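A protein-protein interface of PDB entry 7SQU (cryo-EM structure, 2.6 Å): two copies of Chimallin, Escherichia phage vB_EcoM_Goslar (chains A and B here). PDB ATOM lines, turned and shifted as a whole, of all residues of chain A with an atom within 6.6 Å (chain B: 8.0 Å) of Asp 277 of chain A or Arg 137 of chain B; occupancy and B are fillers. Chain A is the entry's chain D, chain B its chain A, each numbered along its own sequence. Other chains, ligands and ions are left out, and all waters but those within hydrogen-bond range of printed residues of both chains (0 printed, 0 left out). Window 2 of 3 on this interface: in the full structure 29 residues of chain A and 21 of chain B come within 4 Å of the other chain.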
ATOM      1  N   ARG A 272       8.286  19.637  19.445  1.00  0.00           N
ATOM      2  CA  ARG A 272       8.202  18.294  19.997  1.00  0.00           C
ATOM      3  C   ARG A 272       6.829  18.085  20.610  1.00  0.00           C
ATOM      4  O   ARG A 272       6.346  18.941  21.353  1.00  0.00           O
ATOM      5  CB  ARG A 272       9.273  18.042  21.052  1.00  0.00           C
ATOM      6  CG  ARG A 272       9.257  16.621  21.558  1.00  0.00           C
ATOM      7  CD  ARG A 272      10.117  16.446  22.769  1.00  0.00           C
ATOM      8  NE  ARG A 272      11.510  16.233  22.403  1.00  0.00           N
ATOM      9  CZ  ARG A 272      12.509  16.997  22.817  1.00  0.00           C
ATOM     10  NH1 ARG A 272      12.304  18.031  23.612  1.00  0.00           N
ATOM     11  NH2 ARG A 272      13.747  16.718  22.419  1.00  0.00           N
ATOM     12  N   GLN A 273       6.201  16.954  20.307  1.00  0.00           N
ATOM     13  CA  GLN A 273       4.924  16.638  20.924  1.00  0.00           C
ATOM     14  C   GLN A 273       5.139  16.328  22.395  1.00  0.00           C
ATOM     15  O   GLN A 273       6.129  15.706  22.776  1.00  0.00           O
ATOM     16  CB  GLN A 273       4.258  15.454  20.239  1.00  0.00           C
ATOM     17  CG  GLN A 273       3.928  15.685  18.784  1.00  0.00           C
ATOM     18  CD  GLN A 273       2.917  16.769  18.585  1.00  0.00           C
ATOM     19  OE1 GLN A 273       3.166  17.743  17.879  1.00  0.00           O
ATOM     20  NE2 GLN A 273       1.761  16.617  19.207  1.00  0.00           N
ATOM     21  N   ALA A 274       4.191  16.761  23.220  1.00  0.00           N
ATOM     22  CA  ALA A 274       4.356  16.633  24.660  1.00  0.00           C
ATOM     23  C   ALA A 274       4.302  15.181  25.115  1.00  0.00           C
ATOM     24  O   ALA A 274       5.207  14.705  25.807  1.00  0.00           O
ATOM     25  CB  ALA A 274       3.284  17.455  25.377  1.00  0.00           C
ATOM     26  N   MET A 275       3.272  14.452  24.708  1.00  0.00           N
ATOM     27  CA  MET A 275       3.057  13.110  25.226  1.00  0.00           C
ATOM     28  C   MET A 275       3.543  12.020  24.280  1.00  0.00           C
ATOM     29  O   MET A 275       4.097  11.014  24.729  1.00  0.00           O
ATOM     30  CB  MET A 275       1.576  12.902  25.551  1.00  0.00           C
ATOM     31  CG  MET A 275       1.280  11.535  26.120  1.00  0.00           C
ATOM     32  SD  MET A 275       2.409  11.212  27.493  1.00  0.00           S
ATOM     33  CE  MET A 275       1.788   9.658  28.132  1.00  0.00           C
ATOM     34  N   SER A 276       3.336  12.194  22.976  1.00  0.00           N
ATOM     35  CA  SER A 276       3.698  11.197  21.983  1.00  0.00           C
ATOM     36  C   SER A 276       5.149  11.266  21.542  1.00  0.00           C
ATOM     37  O   SER A 276       5.604  10.343  20.866  1.00  0.00           O
ATOM     38  CB  SER A 276       2.801  11.349  20.766  1.00  0.00           C
ATOM     39  OG  SER A 276       2.599  12.718  20.489  1.00  0.00           O
ATOM     40  N   ASP A 277       5.879  12.322  21.890  1.00  0.00           N
ATOM     41  CA  ASP A 277       7.315  12.424  21.643  1.00  0.00           C
ATOM     42  C   ASP A 277       7.708  12.488  20.166  1.00  0.00           C
ATOM     43  O   ASP A 277       8.843  12.162  19.827  1.00  0.00           O
ATOM     44  CB  ASP A 277       8.032  11.247  22.307  1.00  0.00           C
ATOM     45  CG  ASP A 277       9.451  11.550  22.653  1.00  0.00           C
ATOM     46  OD1 ASP A 277       9.727  12.661  23.148  1.00  0.00           O
ATOM     47  OD2 ASP A 277      10.293  10.662  22.440  1.00  0.00           O
ATOM     48  N   TYR A 278       6.825  12.907  19.270  1.00  0.00           N
ATOM     49  CA  TYR A 278       7.199  13.044  17.870  1.00  0.00           C
ATOM     50  C   TYR A 278       8.036  14.301  17.666  1.00  0.00           C
ATOM     51  O   TYR A 278       7.935  15.262  18.424  1.00  0.00           O
ATOM     52  CB  TYR A 278       5.961  13.094  16.977  1.00  0.00           C
ATOM     53  CG  TYR A 278       5.081  11.894  17.122  1.00  0.00           C
ATOM     54  CD1 TYR A 278       5.592  10.687  17.521  1.00  0.00           C
ATOM     55  CD2 TYR A 278       3.739  11.969  16.874  1.00  0.00           C
ATOM     56  CE1 TYR A 278       4.801   9.603  17.668  1.00  0.00           C
ATOM     57  CE2 TYR A 278       2.940  10.884  17.024  1.00  0.00           C
ATOM     58  CZ  TYR A 278       3.476   9.708  17.423  1.00  0.00           C
ATOM     59  OH  TYR A 278       2.678   8.614  17.571  1.00  0.00           O
ATOM     60  N   ASP A 279       8.872  14.290  16.641  1.00  0.00           N
ATOM     61  CA  ASP A 279       9.748  15.410  16.339  1.00  0.00           C
ATOM     62  C   ASP A 279       9.463  15.945  14.948  1.00  0.00           C
ATOM     63  O   ASP A 279       9.256  15.176  14.010  1.00  0.00           O
ATOM     64  CB  ASP A 279      11.212  15.011  16.423  1.00  0.00           C
ATOM     65  CG  ASP A 279      11.786  15.199  17.809  1.00  0.00           C
ATOM     66  OD1 ASP A 279      11.891  16.357  18.264  1.00  0.00           O
ATOM     67  OD2 ASP A 279      12.141  14.189  18.446  1.00  0.00           O
ATOM     68  N   ARG A 583      20.027  28.313  17.653  1.00  0.00           N
ATOM     69  CA  ARG A 583      20.997  27.223  17.723  1.00  0.00           C
ATOM     70  C   ARG A 583      21.355  26.733  16.331  1.00  0.00           C
ATOM     71  O   ARG A 583      20.590  25.963  15.728  1.00  0.00           O
ATOM     72  CB  ARG A 583      20.443  26.073  18.554  1.00  0.00           C
ATOM     73  CG  ARG A 583      21.383  24.911  18.685  1.00  0.00           C
ATOM     74  CD  ARG A 583      20.816  23.853  19.592  1.00  0.00           C
ATOM     75  NE  ARG A 583      19.905  22.959  18.897  1.00  0.00           N
ATOM     76  CZ  ARG A 583      19.001  22.203  19.503  1.00  0.00           C
ATOM     77  NH1 ARG A 583      18.867  22.213  20.818  1.00  0.00           N
ATOM     78  NH2 ARG A 583      18.217  21.416  18.774  1.00  0.00           N
ATOM     79  N   GLU A 585      22.852  24.366  13.542  1.00  0.00           N
ATOM     80  CA  GLU A 585      22.884  22.914  13.584  1.00  0.00           C
ATOM     81  C   GLU A 585      23.894  22.268  12.655  1.00  0.00           C
ATOM     82  O   GLU A 585      24.133  21.064  12.778  1.00  0.00           O
ATOM     83  CB  GLU A 585      21.502  22.347  13.233  1.00  0.00           C
ATOM     84  CG  GLU A 585      20.525  22.321  14.379  1.00  0.00           C
ATOM     85  CD  GLU A 585      19.384  21.352  14.146  1.00  0.00           C
ATOM     86  OE1 GLU A 585      19.241  20.863  13.007  1.00  0.00           O
ATOM     87  OE2 GLU A 585      18.633  21.081  15.106  1.00  0.00           O
ATOM     88  N   SER B 100      -3.527  10.214  16.557  1.00  0.00           N
ATOM     89  CA  SER B 100      -2.233  10.752  16.958  1.00  0.00           C
ATOM     90  C   SER B 100      -1.126  10.001  16.224  1.00  0.00           C
ATOM     91  O   SER B 100      -0.467   9.115  16.765  1.00  0.00           O
ATOM     92  CB  SER B 100      -2.083  10.666  18.467  1.00  0.00           C
ATOM     93  OG  SER B 100      -0.894  11.280  18.899  1.00  0.00           O
ATOM     94  N   LEU B 134      13.501  15.480   9.289  1.00  0.00           N
ATOM     95  CA  LEU B 134      13.589  15.583  10.736  1.00  0.00           C
ATOM     96  C   LEU B 134      14.820  16.377  11.168  1.00  0.00           C
ATOM     97  O   LEU B 134      15.865  16.316  10.523  1.00  0.00           O
ATOM     98  CB  LEU B 134      13.653  14.194  11.350  1.00  0.00           C
ATOM     99  CG  LEU B 134      12.358  13.538  11.814  1.00  0.00           C
ATOM    100  CD1 LEU B 134      11.551  13.110  10.634  1.00  0.00           C
ATOM    101  CD2 LEU B 134      12.661  12.351  12.685  1.00  0.00           C
ATOM    102  N   PRO B 135      14.726  17.110  12.265  1.00  0.00           N
ATOM    103  CA  PRO B 135      15.887  17.816  12.807  1.00  0.00           C
ATOM    104  C   PRO B 135      16.739  16.881  13.658  1.00  0.00           C
ATOM    105  O   PRO B 135      16.393  15.736  13.904  1.00  0.00           O
ATOM    106  CB  PRO B 135      15.248  18.912  13.650  1.00  0.00           C
ATOM    107  CG  PRO B 135      13.994  18.313  14.108  1.00  0.00           C
ATOM    108  CD  PRO B 135      13.513  17.381  13.046  1.00  0.00           C
ATOM    109  N   ARG B 136      17.868  17.399  14.116  1.00  0.00           N
ATOM    110  CA  ARG B 136      18.787  16.630  14.940  1.00  0.00           C
ATOM    111  C   ARG B 136      18.383  16.694  16.399  1.00  0.00           C
ATOM    112  O   ARG B 136      17.845  17.694  16.870  1.00  0.00           O
ATOM    113  CB  ARG B 136      20.209  17.142  14.779  1.00  0.00           C
ATOM    114  CG  ARG B 136      20.886  16.616  13.564  1.00  0.00           C
ATOM    115  CD  ARG B 136      22.362  16.654  13.733  1.00  0.00           C
ATOM    116  NE  ARG B 136      23.028  16.898  12.467  1.00  0.00           N
ATOM    117  CZ  ARG B 136      24.340  16.906  12.305  1.00  0.00           C
ATOM    118  NH1 ARG B 136      25.161  16.670  13.313  1.00  0.00           N
ATOM    119  NH2 ARG B 136      24.843  17.162  11.104  1.00  0.00           N
ATOM    120  N   ARG B 137      18.679  15.627  17.122  1.00  0.00           N
ATOM    121  CA  ARG B 137      18.333  15.506  18.527  1.00  0.00           C
ATOM    122  C   ARG B 137      19.580  15.593  19.391  1.00  0.00           C
ATOM    123  O   ARG B 137      20.601  14.977  19.086  1.00  0.00           O
ATOM    124  CB  ARG B 137      17.621  14.192  18.797  1.00  0.00           C
ATOM    125  CG  ARG B 137      17.007  14.120  20.156  1.00  0.00           C
ATOM    126  CD  ARG B 137      16.233  12.849  20.332  1.00  0.00           C
ATOM    127  NE  ARG B 137      14.821  13.124  20.554  1.00  0.00           N
ATOM    128  CZ  ARG B 137      13.924  12.202  20.864  1.00  0.00           C
ATOM    129  NH1 ARG B 137      14.255  10.932  20.992  1.00  0.00           N
ATOM    130  NH2 ARG B 137      12.662  12.567  21.052  1.00  0.00           N
ATOM    131  N   GLU B 138      19.486  16.345  20.477  1.00  0.00           N
ATOM    132  CA  GLU B 138      20.588  16.500  21.411  1.00  0.00           C
ATOM    133  C   GLU B 138      20.560  15.388  22.448  1.00  0.00           C
ATOM    134  O   GLU B 138      19.527  15.142  23.074  1.00  0.00           O
ATOM    135  CB  GLU B 138      20.513  17.857  22.092  1.00  0.00           C
ATOM    136  CG  GLU B 138      21.264  17.921  23.379  1.00  0.00           C
ATOM    137  CD  GLU B 138      21.425  19.329  23.885  1.00  0.00           C
ATOM    138  OE1 GLU B 138      22.245  20.071  23.311  1.00  0.00           O
ATOM    139  OE2 GLU B 138      20.737  19.697  24.863  1.00  0.00           O
ATOM    140  N   GLU B 139      21.692  14.725  22.631  1.00  0.00           N
ATOM    141  CA  GLU B 139      21.827  13.610  23.551  1.00  0.00           C
ATOM    142  C   GLU B 139      22.895  13.915  24.591  1.00  0.00           C
ATOM    143  O   GLU B 139      23.531  14.969  24.577  1.00  0.00           O
ATOM    144  CB  GLU B 139      22.162  12.326  22.801  1.00  0.00           C
ATOM    145  CG  GLU B 139      21.041  11.834  21.929  1.00  0.00           C
ATOM    146  CD  GLU B 139      21.113  10.350  21.701  1.00  0.00           C
ATOM    147  OE1 GLU B 139      21.742   9.658  22.527  1.00  0.00           O
ATOM    148  OE2 GLU B 139      20.541   9.869  20.700  1.00  0.00           O
ATOM    149  N   GLN B 140      23.093  12.966  25.498  1.00  0.00           N
ATOM    150  CA  GLN B 140      24.040  13.101  26.595  1.00  0.00           C
ATOM    151  C   GLN B 140      25.224  12.175  26.368  1.00  0.00           C
ATOM    152  O   GLN B 140      25.046  10.981  26.111  1.00  0.00           O
ATOM    153  CB  GLN B 140      23.372  12.785  27.929  1.00  0.00           C
ATOM    154  CG  GLN B 140      22.977  14.018  28.705  1.00  0.00           C
ATOM    155  CD  GLN B 140      24.115  15.002  28.838  1.00  0.00           C
ATOM    156  OE1 GLN B 140      25.241  14.627  29.159  1.00  0.00           O
ATOM    157  NE2 GLN B 140      23.825  16.273  28.590  1.00  0.00           N
ATOM    158  N   ASN B 145      27.392  17.202  25.396  1.00  0.00           N
ATOM    159  CA  ASN B 145      26.213  17.000  24.573  1.00  0.00           C
ATOM    160  C   ASN B 145      26.593  16.886  23.106  1.00  0.00           C
ATOM    161  O   ASN B 145      27.474  17.600  22.626  1.00  0.00           O
ATOM    162  CB  ASN B 145      25.216  18.137  24.755  1.00  0.00           C
ATOM    163  CG  ASN B 145      24.795  18.304  26.189  1.00  0.00           C
ATOM    164  OD1 ASN B 145      24.974  17.400  27.004  1.00  0.00           O
ATOM    165  ND2 ASN B 145      24.221  19.452  26.508  1.00  0.00           N
ATOM    166  N   ILE B 146      25.915  15.987  22.401  1.00  0.00           N
ATOM    167  CA  ILE B 146      26.136  15.782  20.981  1.00  0.00           C
ATOM    168  C   ILE B 146      24.789  15.830  20.279  1.00  0.00           C
ATOM    169  O   ILE B 146      23.747  15.581  20.878  1.00  0.00           O
ATOM    170  CB  ILE B 146      26.847  14.449  20.697  1.00  0.00           C
ATOM    171  CG1 ILE B 146      26.162  13.310  21.442  1.00  0.00           C
ATOM    172  CG2 ILE B 146      28.270  14.521  21.147  1.00  0.00           C
ATOM    173  CD1 ILE B 146      26.746  11.967  21.138  1.00  0.00           C
ATOM    174  N   LEU B 147      24.820  16.168  18.997  1.00  0.00           N
ATOM    175  CA  LEU B 147      23.631  16.243  18.161  1.00  0.00           C
ATOM    176  C   LEU B 147      23.645  15.064  17.201  1.00  0.00           C
ATOM    177  O   LEU B 147      24.571  14.932  16.404  1.00  0.00           O
ATOM    178  CB  LEU B 147      23.582  17.564  17.407  1.00  0.00           C
ATOM    179  CG  LEU B 147      23.410  18.813  18.265  1.00  0.00           C
ATOM    180  CD1 LEU B 147      23.814  20.040  17.505  1.00  0.00           C
ATOM    181  CD2 LEU B 147      21.985  18.941  18.712  1.00  0.00           C
ATOM    182  N   VAL B 148      22.608  14.247  17.249  1.00  0.00           N
ATOM    183  CA  VAL B 148      22.568  12.961  16.557  1.00  0.00           C
ATOM    184  C   VAL B 148      21.559  13.034  15.424  1.00  0.00           C
ATOM    185  O   VAL B 148      20.444  13.517  15.634  1.00  0.00           O
ATOM    186  CB  VAL B 148      22.218  11.820  17.524  1.00  0.00           C
ATOM    187  CG1 VAL B 148      22.420  10.490  16.863  1.00  0.00           C
ATOM    188  CG2 VAL B 148      23.067  11.925  18.760  1.00  0.00           C
ATOM    189  N   PRO B 149      21.898  12.571  14.222  1.00  0.00           N
ATOM    190  CA  PRO B 149      20.940  12.600  13.112  1.00  0.00           C
ATOM    191  C   PRO B 149      19.785  11.630  13.299  1.00  0.00           C
ATOM    192  O   PRO B 149      19.912  10.594  13.946  1.00  0.00           O
ATOM    193  CB  PRO B 149      21.792  12.182  11.911  1.00  0.00           C
ATOM    194  CG  PRO B 149      23.171  12.300  12.348  1.00  0.00           C
ATOM    195  CD  PRO B 149      23.210  12.079  13.792  1.00  0.00           C
ATOM    196  N   ARG B 150      18.647  11.973  12.695  1.00  0.00           N
ATOM    197  CA  ARG B 150      17.464  11.124  12.700  1.00  0.00           C
ATOM    198  C   ARG B 150      16.876  11.049  11.300  1.00  0.00           C
ATOM    199  O   ARG B 150      17.170  11.875  10.439  1.00  0.00           O
ATOM    200  CB  ARG B 150      16.383  11.634  13.648  1.00  0.00           C
ATOM    201  CG  ARG B 150      16.836  12.587  14.694  1.00  0.00           C
ATOM    202  CD  ARG B 150      17.288  11.899  15.949  1.00  0.00           C
ATOM    203  NE  ARG B 150      16.401  10.836  16.404  1.00  0.00           N
ATOM    204  CZ  ARG B 150      15.222  11.026  16.978  1.00  0.00           C
ATOM    205  NH1 ARG B 150      14.728  12.236  17.161  1.00  0.00           N
ATOM    206  NH2 ARG B 150      14.531   9.975  17.406  1.00  0.00           N
ATOM    207  N   ASP B 154      12.583   6.914  12.888  1.00  0.00           N
ATOM    208  CA  ASP B 154      12.779   7.204  14.301  1.00  0.00           C
ATOM    209  C   ASP B 154      11.519   7.699  14.993  1.00  0.00           C
ATOM    210  O   ASP B 154      11.499   7.746  16.222  1.00  0.00           O
ATOM    211  CB  ASP B 154      13.888   8.232  14.481  1.00  0.00           C
ATOM    212  CG  ASP B 154      15.260   7.660  14.229  1.00  0.00           C
ATOM    213  OD1 ASP B 154      15.615   6.647  14.855  1.00  0.00           O
ATOM    214  OD2 ASP B 154      15.992   8.225  13.402  1.00  0.00           O
ATOM    215  N   ASN B 155      10.480   8.064  14.252  1.00  0.00           N
ATOM    216  CA  ASN B 155       9.246   8.566  14.838  1.00  0.00           C
ATOM    217  C   ASN B 155       8.193   7.486  15.027  1.00  0.00           C
ATOM    218  O   ASN B 155       7.112   7.786  15.524  1.00  0.00           O
ATOM    219  CB  ASN B 155       8.663   9.666  13.964  1.00  0.00           C
ATOM    220  CG  ASN B 155       9.005  11.038  14.447  1.00  0.00           C
ATOM    221  OD1 ASN B 155       9.456  11.220  15.565  1.00  0.00           O
ATOM    222  ND2 ASN B 155       8.796  12.020  13.603  1.00  0.00           N
ATOM    223  N   LEU B 156       8.477   6.245  14.653  1.00  0.00           N
ATOM    224  CA  LEU B 156       7.488   5.174  14.724  1.00  0.00           C
ATOM    225  C   LEU B 156       7.718   4.379  16.006  1.00  0.00           C
ATOM    226  O   LEU B 156       8.340   3.325  16.017  1.00  0.00           O
ATOM    227  CB  LEU B 156       7.564   4.306  13.478  1.00  0.00           C
ATOM    228  CG  LEU B 156       7.480   5.112  12.178  1.00  0.00           C
ATOM    229  CD1 LEU B 156       7.576   4.228  10.973  1.00  0.00           C
ATOM    230  CD2 LEU B 156       6.209   5.920  12.124  1.00  0.00           C
ATOM    231  N   ASN B 157       7.165   4.892  17.096  1.00  0.00           N
ATOM    232  CA  ASN B 157       7.305   4.328  18.425  1.00  0.00           C
ATOM    233  C   ASN B 157       6.032   3.582  18.833  1.00  0.00           C
ATOM    234  O   ASN B 157       5.183   3.264  18.003  1.00  0.00           O
ATOM    235  CB  ASN B 157       7.663   5.425  19.423  1.00  0.00           C
ATOM    236  CG  ASN B 157       6.808   6.650  19.278  1.00  0.00           C
ATOM    237  OD1 ASN B 157       5.643   6.564  18.927  1.00  0.00           O
ATOM    238  ND2 ASN B 157       7.376   7.803  19.567  1.00  0.00           N
ATOM    239  N   THR B 159       3.464   4.542  20.637  1.00  0.00           N
ATOM    240  CA  THR B 159       2.228   5.306  20.495  1.00  0.00           C
ATOM    241  C   THR B 159       1.643   5.146  19.100  1.00  0.00           C
ATOM    242  O   THR B 159       0.424   5.010  18.934  1.00  0.00           O
ATOM    243  CB  THR B 159       2.499   6.779  20.788  1.00  0.00           C
ATOM    244  OG1 THR B 159       3.273   6.886  21.982  1.00  0.00           O
ATOM    245  CG2 THR B 159       1.220   7.536  20.964  1.00  0.00           C
ATOM    246  N   SER B 534      25.706   6.062  19.494  1.00  0.00           N
ATOM    247  CA  SER B 534      25.488   7.405  18.975  1.00  0.00           C
ATOM    248  C   SER B 534      26.801   8.064  18.572  1.00  0.00           C
ATOM    249  O   SER B 534      26.853   8.797  17.581  1.00  0.00           O
ATOM    250  CB  SER B 534      24.730   8.243  19.996  1.00  0.00           C
ATOM    251  OG  SER B 534      25.371   8.209  21.250  1.00  0.00           O
ATOM    252  N   VAL B 538      27.684   9.541  14.874  1.00  0.00           N
ATOM    253  CA  VAL B 538      28.097  10.925  14.660  1.00  0.00           C
ATOM    254  C   VAL B 538      29.402  10.993  13.877  1.00  0.00           C
ATOM    255  O   VAL B 538      29.543  11.802  12.949  1.00  0.00           O
ATOM    256  CB  VAL B 538      28.201  11.654  16.010  1.00  0.00           C
ATOM    257  CG1 VAL B 538      28.949  12.934  15.861  1.00  0.00           C
ATOM    258  CG2 VAL B 538      26.833  11.921  16.556  1.00  0.00           C
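CE1 of Tyr 278 of chain A touches O of Asn 155 of chain B (3.6 Å).
Tyr 278 of chain A touches Asn 157 of chain B (CE1 to OD1, 3.4 Å).
CB of Thr 159 of chain B touches OH of Tyr 278 of chain A, at 3.7 Å.
Arg 136 of chain B touches Glu 585 of chain A (N to OE1, 3.9 Å).
Of the printed residues of chain B, Asp 277 of chain A touches Arg 137.
Arg 137 of chain B touches two residues of chain A.
Ser 276 of chain A touches one residue of chain B.
Of the printed residues of chain B, Glu 585 of chain A touches Arg 136.
Of the printed residues of chain A, Arg 150 of chain B touches Asp 279.
The nearest printed residue of chain B that does not touch Tyr 278 of chain A is Leu 156 of chain B (5.8 Å).
The backbone carbonyl oxygen (O) of Ser 100 of chain B sits at hydrogen-bond distance from the side-chain hydroxyl (OH) of Tyr 278 of chain A (3.3 Å).
NH2 of Arg 137 of chain B lies within salt-bridge range of OD2 of Asp 277 of chain A, at 3.3 Å.
The guanidinium group (NH2) of Arg 137 of chain B is in salt-bridge range of the side-chain carboxylate (OD2) of Asp 279 of chain A (3.1 Å).
NH1 of Arg 150 of chain B is in salt-bridge range of OD2 of Asp 279 of chain A (3.5 Å).
ND2 of Asn 155 of chain B sits at hydrogen-bond distance from O of Asp 279 of chain A (3.2 Å).
O of Ser 276 of chain A sits at hydrogen-bond distance from ND2 of Asn 157 of chain B (3.4 Å).
No position is printed for both chains.
The backbone NH (N) of Val 148 of chain B sits at hydrogen-bond distance from the backbone carbonyl oxygen (O) of Arg 137 of chain B.
The backbone NH (N) of Thr 159 of chain B lies close to the side-chain amide oxygen (OD1) of Asn 157 of chain B.
The backbone NH (N) of Gln 273 of chain A sits at hydrogen-bond distance from the backbone carbonyl oxygen (O) of Tyr 278 of chain A (3.1 Å).
The guanidinium group of Arg 583 of chain A is in salt-bridge range of the side-chain carboxylate of Glu 585 of chain A.
Of the 10 printed residues of chain A, 5 touch a printed residue of chain B.
Hydrophobic or aromatic side chains of chain A within 4 Å of the printed part of chain B: Tyr 278.
Along chain A the printed residues that touch a printed residue of chain B span positions 276 to 585.
Printed residues of chain B that touch a printed residue of chain A: Ser 100, Arg 136, Arg 137, Arg 150, Asn 155, Asn 157 and Thr 159.
Among the printed residues, Asp or Glu carboxylates within 4 Å of a Lys or Arg side-chain nitrogen of the other chain: Asp 277 of chain A with Arg 137 of chain B (3.3 Å), Asp 279 of chain A with Arg 137 of chain B (3.1 Å) and Asp 279 of chain A with Arg 150 of chain B (3.5 Å).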
